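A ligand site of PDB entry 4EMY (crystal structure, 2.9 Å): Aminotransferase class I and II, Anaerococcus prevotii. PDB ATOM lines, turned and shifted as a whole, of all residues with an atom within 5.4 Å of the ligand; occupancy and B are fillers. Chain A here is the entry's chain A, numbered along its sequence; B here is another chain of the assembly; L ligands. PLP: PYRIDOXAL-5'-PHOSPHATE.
N of Gly 110 lies within hydrogen-bond range of O2P of the ligand (2.8 Å). OH of Tyr 227 lies within hydrogen-bond range of O3 of the ligand (2.6 Å). An oxygen (O3) of the ligand is in hydrogen-bond range of the side-chain amide nitrogen of Asn 190 (2.7 Å). An oxygen (O1P) of the ligand lies within hydrogen-bond range of the backbone NH (N) of Thr 111 (3.0 Å). The guanidinium group of Arg 269 lies within salt-bridge range of an oxygen (O1P) of the ligand. OD2 of Asp 224 is in hydrogen-bond range of N1 of the ligand (2.5 Å). OG of Ser 260 lies within hydrogen-bond range of O2P of the ligand, at 2.5 Å. OG of Ser 258 sits at hydrogen-bond distance from O2P of the ligand, at 2.6 Å. The side-chain hydroxyl (OH) of Tyr 75 of chain B is in hydrogen-bond range of an oxygen (O3P) of the ligand, 2.6 Å away. The side-chain hydroxyl of Thr 111 sits at hydrogen-bond distance from an oxygen (O1P) of the ligand (2.7 Å). The side-chain amino group (NZ) of Lys 261 is in hydrogen-bond range of an oxygen (O4A) of the ligand (2.8 Å).
The guanidinium group (NH2) of Arg 269 is in hydrogen-bond range of the backbone carbonyl oxygen (O) of Trp 298 of chain B (2.9 Å). The side-chain hydroxyl (OG1) of Thr 111 sits at hydrogen-bond distance from the side-chain hydroxyl (OG) of Ser 299 of chain B (3.3 Å). O of Pro 108 lies within hydrogen-bond range of NH2 of Arg 269 (3.1 Å). The backbone NH (N) of Ala 226 is in hydrogen-bond range of the side-chain carboxylate (OD1) of Asp 224 (3.4 Å). The guanidinium group (NH1) of Arg 269 lies close to the backbone carbonyl oxygen (O) of Tyr 266, at 3.3 Å. The side-chain hydroxyl (OG) of Ser 258 is in hydrogen-bond range of the backbone NH (N) of Ser 260, at 3.0 Å. The side-chain carboxylate (OD2) of Asp 224 is in hydrogen-bond range of the side-chain hydroxyl (OH) of Tyr 138, 2.4 Å away. The backbone carbonyl oxygen of Asp 224 sits at hydrogen-bond distance from the side-chain amide nitrogen of Asn 185, at 2.7 Å.
Residues that only touch the ligand: Asn 185, Gly 109, Trp 135 and Tyr 138. Hydrophobic or aromatic side chains that line the ligand: Trp 135, Tyr 227 and Tyr 75 of chain B. Of the 24 residues printed, 14 come within 4 Å of the ligand.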
ATOM      1  N   GLY A  45     -21.585   3.520  14.777  1.00  0.00           N
ATOM      2  CA  GLY A  45     -22.558   2.712  14.057  1.00  0.00           C
ATOM      3  C   GLY A  45     -24.008   2.933  14.449  1.00  0.00           C
ATOM      4  O   GLY A  45     -24.636   2.077  15.084  1.00  0.00           O
ATOM      5  N   PRO A 108     -29.933  -9.578  26.184  1.00  0.00           N
ATOM      6  CA  PRO A 108     -29.867  -8.121  26.062  1.00  0.00           C
ATOM      7  C   PRO A 108     -29.048  -7.748  24.817  1.00  0.00           C
ATOM      8  O   PRO A 108     -27.813  -7.732  24.851  1.00  0.00           O
ATOM      9  CB  PRO A 108     -29.187  -7.681  27.375  1.00  0.00           C
ATOM     10  CG  PRO A 108     -28.402  -8.869  27.815  1.00  0.00           C
ATOM     11  CD  PRO A 108     -29.073 -10.100  27.269  1.00  0.00           C
ATOM     12  N   GLY A 109     -29.769  -7.511  23.717  1.00  0.00           N
ATOM     13  CA  GLY A 109     -29.147  -7.295  22.407  1.00  0.00           C
ATOM     14  C   GLY A 109     -28.348  -8.494  21.929  1.00  0.00           C
ATOM     15  O   GLY A 109     -28.410  -9.578  22.514  1.00  0.00           O
ATOM     16  N   GLY A 110     -27.593  -8.304  20.849  1.00  0.00           N
ATOM     17  CA  GLY A 110     -26.729  -9.351  20.329  1.00  0.00           C
ATOM     18  C   GLY A 110     -25.587  -9.648  21.281  1.00  0.00           C
ATOM     19  O   GLY A 110     -25.161 -10.793  21.410  1.00  0.00           O
ATOM     20  N   THR A 111     -25.110  -8.602  21.952  1.00  0.00           N
ATOM     21  CA  THR A 111     -24.066  -8.731  22.962  1.00  0.00           C
ATOM     22  C   THR A 111     -24.401  -9.868  23.933  1.00  0.00           C
ATOM     23  O   THR A 111     -23.551 -10.724  24.234  1.00  0.00           O
ATOM     24  CB  THR A 111     -23.852  -7.401  23.721  1.00  0.00           C
ATOM     25  OG1 THR A 111     -23.479  -6.369  22.798  1.00  0.00           O
ATOM     26  CG2 THR A 111     -22.765  -7.533  24.791  1.00  0.00           C
ATOM     27  N   GLY A 112     -25.653  -9.874  24.404  1.00  0.00           N
ATOM     28  CA  GLY A 112     -26.151 -10.915  25.291  1.00  0.00           C
ATOM     29  C   GLY A 112     -25.940 -12.315  24.740  1.00  0.00           C
ATOM     30  O   GLY A 112     -25.466 -13.217  25.441  1.00  0.00           O
ATOM     31  N   ILE A 114     -23.797 -13.303  22.360  1.00  0.00           N
ATOM     32  CA  ILE A 114     -22.400 -13.649  22.108  1.00  0.00           C
ATOM     33  C   ILE A 114     -21.667 -14.097  23.370  1.00  0.00           C
ATOM     34  O   ILE A 114     -20.987 -15.124  23.359  1.00  0.00           O
ATOM     35  CB  ILE A 114     -21.644 -12.493  21.413  1.00  0.00           C
ATOM     36  CG1 ILE A 114     -22.031 -12.451  19.943  1.00  0.00           C
ATOM     37  CG2 ILE A 114     -20.131 -12.653  21.528  1.00  0.00           C
ATOM     38  CD1 ILE A 114     -21.575 -11.192  19.256  1.00  0.00           C
ATOM     39  N   TRP A 135     -14.876  -6.704  15.975  1.00  0.00           N
ATOM     40  CA  TRP A 135     -15.543  -5.836  16.934  1.00  0.00           C
ATOM     41  C   TRP A 135     -14.925  -6.095  18.275  1.00  0.00           C
ATOM     42  O   TRP A 135     -14.925  -7.221  18.761  1.00  0.00           O
ATOM     43  CB  TRP A 135     -17.029  -6.174  16.920  1.00  0.00           C
ATOM     44  CG  TRP A 135     -17.911  -5.358  17.822  1.00  0.00           C
ATOM     45  CD1 TRP A 135     -17.946  -3.980  17.976  1.00  0.00           C
ATOM     46  CD2 TRP A 135     -18.984  -5.862  18.701  1.00  0.00           C
ATOM     47  NE1 TRP A 135     -18.916  -3.604  18.869  1.00  0.00           N
ATOM     48  CE2 TRP A 135     -19.569  -4.683  19.342  1.00  0.00           C
ATOM     49  CE3 TRP A 135     -19.483  -7.115  19.012  1.00  0.00           C
ATOM     50  CZ2 TRP A 135     -20.610  -4.778  20.254  1.00  0.00           C
ATOM     51  CZ3 TRP A 135     -20.530  -7.213  19.932  1.00  0.00           C
ATOM     52  CH2 TRP A 135     -21.083  -6.064  20.535  1.00  0.00           C
ATOM     53  N   TYR A 138     -15.514  -8.790  21.418  1.00  0.00           N
ATOM     54  CA  TYR A 138     -15.253 -10.239  21.326  1.00  0.00           C
ATOM     55  C   TYR A 138     -14.055 -10.629  22.211  1.00  0.00           C
ATOM     56  O   TYR A 138     -14.118 -11.581  22.984  1.00  0.00           O
ATOM     57  CB  TYR A 138     -14.984 -10.711  19.897  1.00  0.00           C
ATOM     58  CG  TYR A 138     -16.099 -10.516  18.893  1.00  0.00           C
ATOM     59  CD1 TYR A 138     -17.409 -10.888  19.192  1.00  0.00           C
ATOM     60  CD2 TYR A 138     -15.838 -10.002  17.623  1.00  0.00           C
ATOM     61  CE1 TYR A 138     -18.426 -10.711  18.260  1.00  0.00           C
ATOM     62  CE2 TYR A 138     -16.842  -9.829  16.686  1.00  0.00           C
ATOM     63  CZ  TYR A 138     -18.139 -10.189  17.014  1.00  0.00           C
ATOM     64  OH  TYR A 138     -19.138 -10.018  16.093  1.00  0.00           O
ATOM     65  N   ASN A 185     -18.273 -12.952  12.136  1.00  0.00           N
ATOM     66  CA  ASN A 185     -19.219 -11.855  12.012  1.00  0.00           C
ATOM     67  C   ASN A 185     -19.501 -11.573  10.536  1.00  0.00           C
ATOM     68  O   ASN A 185     -18.767 -10.845   9.875  1.00  0.00           O
ATOM     69  CB  ASN A 185     -18.700 -10.607  12.735  1.00  0.00           C
ATOM     70  CG  ASN A 185     -19.630  -9.419  12.576  1.00  0.00           C
ATOM     71  OD1 ASN A 185     -19.179  -8.277  12.453  1.00  0.00           O
ATOM     72  ND2 ASN A 185     -20.939  -9.670  12.587  1.00  0.00           N
ATOM     73  N   ASN A 190     -18.558  -5.817  10.789  1.00  0.00           N
ATOM     74  CA  ASN A 190     -17.983  -4.644  11.424  1.00  0.00           C
ATOM     75  C   ASN A 190     -16.552  -5.021  11.862  1.00  0.00           C
ATOM     76  O   ASN A 190     -16.393  -5.953  12.674  1.00  0.00           O
ATOM     77  CB  ASN A 190     -18.874  -4.234  12.602  1.00  0.00           C
ATOM     78  CG  ASN A 190     -18.218  -3.257  13.538  1.00  0.00           C
ATOM     79  OD1 ASN A 190     -17.471  -2.379  13.137  1.00  0.00           O
ATOM     80  ND2 ASN A 190     -18.508  -3.405  14.817  1.00  0.00           N
ATOM     81  N   ASP A 224     -22.268 -13.923  14.157  1.00  0.00           N
ATOM     82  CA  ASP A 224     -22.835 -12.633  14.546  1.00  0.00           C
ATOM     83  C   ASP A 224     -23.560 -12.027  13.346  1.00  0.00           C
ATOM     84  O   ASP A 224     -22.938 -11.485  12.439  1.00  0.00           O
ATOM     85  CB  ASP A 224     -21.739 -11.695  15.052  1.00  0.00           C
ATOM     86  CG  ASP A 224     -22.296 -10.437  15.768  1.00  0.00           C
ATOM     87  OD1 ASP A 224     -23.495 -10.113  15.641  1.00  0.00           O
ATOM     88  OD2 ASP A 224     -21.502  -9.768  16.457  1.00  0.00           O
ATOM     89  N   ALA A 226     -25.860  -9.499  13.285  1.00  0.00           N
ATOM     90  CA  ALA A 226     -26.508  -8.233  13.641  1.00  0.00           C
ATOM     91  C   ALA A 226     -26.879  -7.385  12.408  1.00  0.00           C
ATOM     92  O   ALA A 226     -27.955  -6.790  12.365  1.00  0.00           O
ATOM     93  CB  ALA A 226     -25.609  -7.440  14.588  1.00  0.00           C
ATOM     94  N   TYR A 227     -25.994  -7.335  11.422  1.00  0.00           N
ATOM     95  CA  TYR A 227     -26.204  -6.514  10.227  1.00  0.00           C
ATOM     96  C   TYR A 227     -26.790  -7.326   9.073  1.00  0.00           C
ATOM     97  O   TYR A 227     -26.635  -6.962   7.906  1.00  0.00           O
ATOM     98  CB  TYR A 227     -24.910  -5.828   9.799  1.00  0.00           C
ATOM     99  CG  TYR A 227     -24.260  -5.013  10.885  1.00  0.00           C
ATOM    100  CD1 TYR A 227     -24.681  -3.702  11.160  1.00  0.00           C
ATOM    101  CD2 TYR A 227     -23.211  -5.529  11.634  1.00  0.00           C
ATOM    102  CE1 TYR A 227     -24.079  -2.946  12.162  1.00  0.00           C
ATOM    103  CE2 TYR A 227     -22.601  -4.784  12.626  1.00  0.00           C
ATOM    104  CZ  TYR A 227     -23.033  -3.504  12.894  1.00  0.00           C
ATOM    105  OH  TYR A 227     -22.418  -2.787  13.881  1.00  0.00           O
ATOM    106  N   SER A 258     -30.019  -9.865  16.600  1.00  0.00           N
ATOM    107  CA  SER A 258     -30.254  -8.568  17.242  1.00  0.00           C
ATOM    108  C   SER A 258     -31.350  -7.725  16.581  1.00  0.00           C
ATOM    109  O   SER A 258     -31.470  -7.673  15.353  1.00  0.00           O
ATOM    110  CB  SER A 258     -28.958  -7.770  17.302  1.00  0.00           C
ATOM    111  OG  SER A 258     -29.149  -6.559  18.016  1.00  0.00           O
ATOM    112  N   MET A 259     -32.134  -7.038  17.411  1.00  0.00           N
ATOM    113  CA  MET A 259     -33.100  -6.063  16.912  1.00  0.00           C
ATOM    114  C   MET A 259     -32.480  -4.684  16.794  1.00  0.00           C
ATOM    115  O   MET A 259     -33.099  -3.773  16.205  1.00  0.00           O
ATOM    116  CB  MET A 259     -34.323  -5.995  17.829  1.00  0.00           C
ATOM    117  CG  MET A 259     -35.334  -7.060  17.572  1.00  0.00           C
ATOM    118  SD  MET A 259     -36.665  -7.056  18.976  1.00  0.00           S
ATOM    119  CE  MET A 259     -37.904  -5.700  18.246  1.00  0.00           C
ATOM    120  N   SER A 260     -31.279  -4.535  17.350  1.00  0.00           N
ATOM    121  CA  SER A 260     -30.621  -3.237  17.458  1.00  0.00           C
ATOM    122  C   SER A 260     -30.590  -2.466  16.148  1.00  0.00           C
ATOM    123  O   SER A 260     -30.961  -1.298  16.108  1.00  0.00           O
ATOM    124  CB  SER A 260     -29.215  -3.396  18.032  1.00  0.00           C
ATOM    125  OG  SER A 260     -29.260  -3.713  19.408  1.00  0.00           O
ATOM    126  N   LYS A 261     -30.167  -3.129  15.065  1.00  0.00           N
ATOM    127  CA  LYS A 261     -30.028  -2.480  13.772  1.00  0.00           C
ATOM    128  C   LYS A 261     -31.252  -2.654  12.898  1.00  0.00           C
ATOM    129  O   LYS A 261     -31.793  -1.680  12.366  1.00  0.00           O
ATOM    130  CB  LYS A 261     -28.792  -3.005  13.039  1.00  0.00           C
ATOM    131  CG  LYS A 261     -27.488  -2.415  13.538  1.00  0.00           C
ATOM    132  CD  LYS A 261     -26.918  -3.197  14.701  1.00  0.00           C
ATOM    133  CE  LYS A 261     -25.829  -2.401  15.402  1.00  0.00           C
ATOM    134  NZ  LYS A 261     -25.075  -3.241  16.362  1.00  0.00           N
ATOM    135  N   TYR A 266     -31.673  -0.021  19.314  1.00  0.00           N
ATOM    136  CA  TYR A 266     -30.429  -0.172  20.065  1.00  0.00           C
ATOM    137  C   TYR A 266     -30.631  -0.017  21.571  1.00  0.00           C
ATOM    138  O   TYR A 266     -30.167  -0.863  22.350  1.00  0.00           O
ATOM    139  CB  TYR A 266     -29.378   0.850  19.598  1.00  0.00           C
ATOM    140  CG  TYR A 266     -29.429   1.219  18.123  1.00  0.00           C
ATOM    141  CD1 TYR A 266     -28.459   0.740  17.234  1.00  0.00           C
ATOM    142  CD2 TYR A 266     -30.422   2.079  17.629  1.00  0.00           C
ATOM    143  CE1 TYR A 266     -28.494   1.095  15.887  1.00  0.00           C
ATOM    144  CE2 TYR A 266     -30.463   2.431  16.289  1.00  0.00           C
ATOM    145  CZ  TYR A 266     -29.499   1.940  15.419  1.00  0.00           C
ATOM    146  OH  TYR A 266     -29.554   2.301  14.097  1.00  0.00           O
ATOM    147  N   ARG A 269     -32.334  -2.776  23.834  1.00  0.00           N
ATOM    148  CA  ARG A 269     -31.558  -3.960  24.242  1.00  0.00           C
ATOM    149  C   ARG A 269     -32.285  -5.294  24.106  1.00  0.00           C
ATOM    150  O   ARG A 269     -32.589  -5.948  25.108  1.00  0.00           O
ATOM    151  CB  ARG A 269     -31.050  -3.803  25.678  1.00  0.00           C
ATOM    152  CG  ARG A 269     -30.353  -2.478  25.986  1.00  0.00           C
ATOM    153  CD  ARG A 269     -29.146  -2.232  25.098  1.00  0.00           C
ATOM    154  NE  ARG A 269     -28.227  -3.381  25.011  1.00  0.00           N
ATOM    155  CZ  ARG A 269     -27.789  -3.906  23.869  1.00  0.00           C
ATOM    156  NH1 ARG A 269     -28.168  -3.409  22.707  1.00  0.00           N
ATOM    157  NH2 ARG A 269     -26.961  -4.926  23.900  1.00  0.00           N
ATOM    158  N   PHE A 358     -20.405   0.045   7.895  1.00  0.00           N
ATOM    159  CA  PHE A 358     -19.087   0.636   7.756  1.00  0.00           C
ATOM    160  C   PHE A 358     -18.431   0.174   6.466  1.00  0.00           C
ATOM    161  O   PHE A 358     -18.616  -0.976   6.057  1.00  0.00           O
ATOM    162  CB  PHE A 358     -18.195   0.230   8.921  1.00  0.00           C
ATOM    163  CG  PHE A 358     -18.841   0.338  10.270  1.00  0.00           C
ATOM    164  CD1 PHE A 358     -19.468  -0.771  10.846  1.00  0.00           C
ATOM    165  CD2 PHE A 358     -18.818   1.539  10.979  1.00  0.00           C
ATOM    166  CE1 PHE A 358     -20.068  -0.678  12.094  1.00  0.00           C
ATOM    167  CE2 PHE A 358     -19.418   1.632  12.226  1.00  0.00           C
ATOM    168  CZ  PHE A 358     -20.037   0.521  12.782  1.00  0.00           C
ATOM    169  N   TYR B  75     -28.384   4.325  21.778  1.00  0.00           N
ATOM    170  CA  TYR B  75     -27.664   3.659  22.863  1.00  0.00           C
ATOM    171  C   TYR B  75     -27.507   4.584  24.072  1.00  0.00           C
ATOM    172  O   TYR B  75     -27.241   5.773  23.938  1.00  0.00           O
ATOM    173  CB  TYR B  75     -26.261   3.228  22.415  1.00  0.00           C
ATOM    174  CG  TYR B  75     -26.178   1.998  21.542  1.00  0.00           C
ATOM    175  CD1 TYR B  75     -26.589   0.744  22.015  1.00  0.00           C
ATOM    176  CD2 TYR B  75     -25.650   2.068  20.253  1.00  0.00           C
ATOM    177  CE1 TYR B  75     -26.499  -0.396  21.219  1.00  0.00           C
ATOM    178  CE2 TYR B  75     -25.567   0.934  19.454  1.00  0.00           C
ATOM    179  CZ  TYR B  75     -25.985  -0.288  19.945  1.00  0.00           C
ATOM    180  OH  TYR B  75     -25.898  -1.406  19.141  1.00  0.00           O
ATOM    181  N   TRP B 298     -24.131  -7.084  28.912  1.00  0.00           N
ATOM    182  CA  TRP B 298     -25.355  -6.516  28.332  1.00  0.00           C
ATOM    183  C   TRP B 298     -25.105  -5.378  27.388  1.00  0.00           C
ATOM    184  O   TRP B 298     -26.006  -4.975  26.651  1.00  0.00           O
ATOM    185  CB  TRP B 298     -26.325  -6.061  29.425  1.00  0.00           C
ATOM    186  CG  TRP B 298     -25.697  -5.168  30.468  1.00  0.00           C
ATOM    187  CD1 TRP B 298     -25.542  -3.782  30.419  1.00  0.00           C
ATOM    188  CD2 TRP B 298     -25.126  -5.573  31.761  1.00  0.00           C
ATOM    189  NE1 TRP B 298     -24.935  -3.316  31.563  1.00  0.00           N
ATOM    190  CE2 TRP B 298     -24.662  -4.342  32.407  1.00  0.00           C
ATOM    191  CE3 TRP B 298     -24.977  -6.784  32.416  1.00  0.00           C
ATOM    192  CZ2 TRP B 298     -24.069  -4.353  33.655  1.00  0.00           C
ATOM    193  CZ3 TRP B 298     -24.375  -6.781  33.676  1.00  0.00           C
ATOM    194  CH2 TRP B 298     -23.931  -5.590  34.279  1.00  0.00           C
ATOM    195  N   SER B 299     -23.887  -4.859  27.410  1.00  0.00           N
ATOM    196  CA  SER B 299     -23.428  -3.766  26.523  1.00  0.00           C
ATOM    197  C   SER B 299     -23.714  -2.400  27.135  1.00  0.00           C
ATOM    198  O   SER B 299     -22.791  -1.622  27.355  1.00  0.00           O
ATOM    199  CB  SER B 299     -24.028  -3.880  25.121  1.00  0.00           C
ATOM    200  OG  SER B 299     -23.145  -3.357  24.150  1.00  0.00           O
HETATM  201  N1  PLP L   1     -22.177  -7.392  16.922  1.00  0.00           N
HETATM  202  C2  PLP L   1     -21.490  -6.543  16.079  1.00  0.00           C
HETATM  203  C2A PLP L   1     -20.544  -7.096  15.054  1.00  0.00           C
HETATM  204  C3  PLP L   1     -21.663  -5.157  16.167  1.00  0.00           C
HETATM  205  O3  PLP L   1     -20.974  -4.326  15.345  1.00  0.00           O
HETATM  206  C4  PLP L   1     -22.518  -4.613  17.102  1.00  0.00           C
HETATM  207  C4A PLP L   1     -22.119  -3.267  17.656  1.00  0.00           C
HETATM  208  O4A PLP L   1     -22.638  -2.226  17.218  1.00  0.00           O
HETATM  209  C5  PLP L   1     -23.219  -5.479  17.941  1.00  0.00           C
HETATM  210  C6  PLP L   1     -23.046  -6.865  17.854  1.00  0.00           C
HETATM  211  C5A PLP L   1     -24.150  -4.884  18.992  1.00  0.00           C
HETATM  212  O4P PLP L   1     -25.313  -5.658  19.205  1.00  0.00           O
HETATM  213  P   PLP L   1     -26.312  -5.151  20.344  1.00  0.00           P
HETATM  214  O1P PLP L   1     -25.786  -5.705  21.643  1.00  0.00           O
HETATM  215  O2P PLP L   1     -27.700  -5.634  20.001  1.00  0.00           O
HETATM  216  O3P PLP L   1     -26.306  -3.643  20.430  1.00  0.00           O
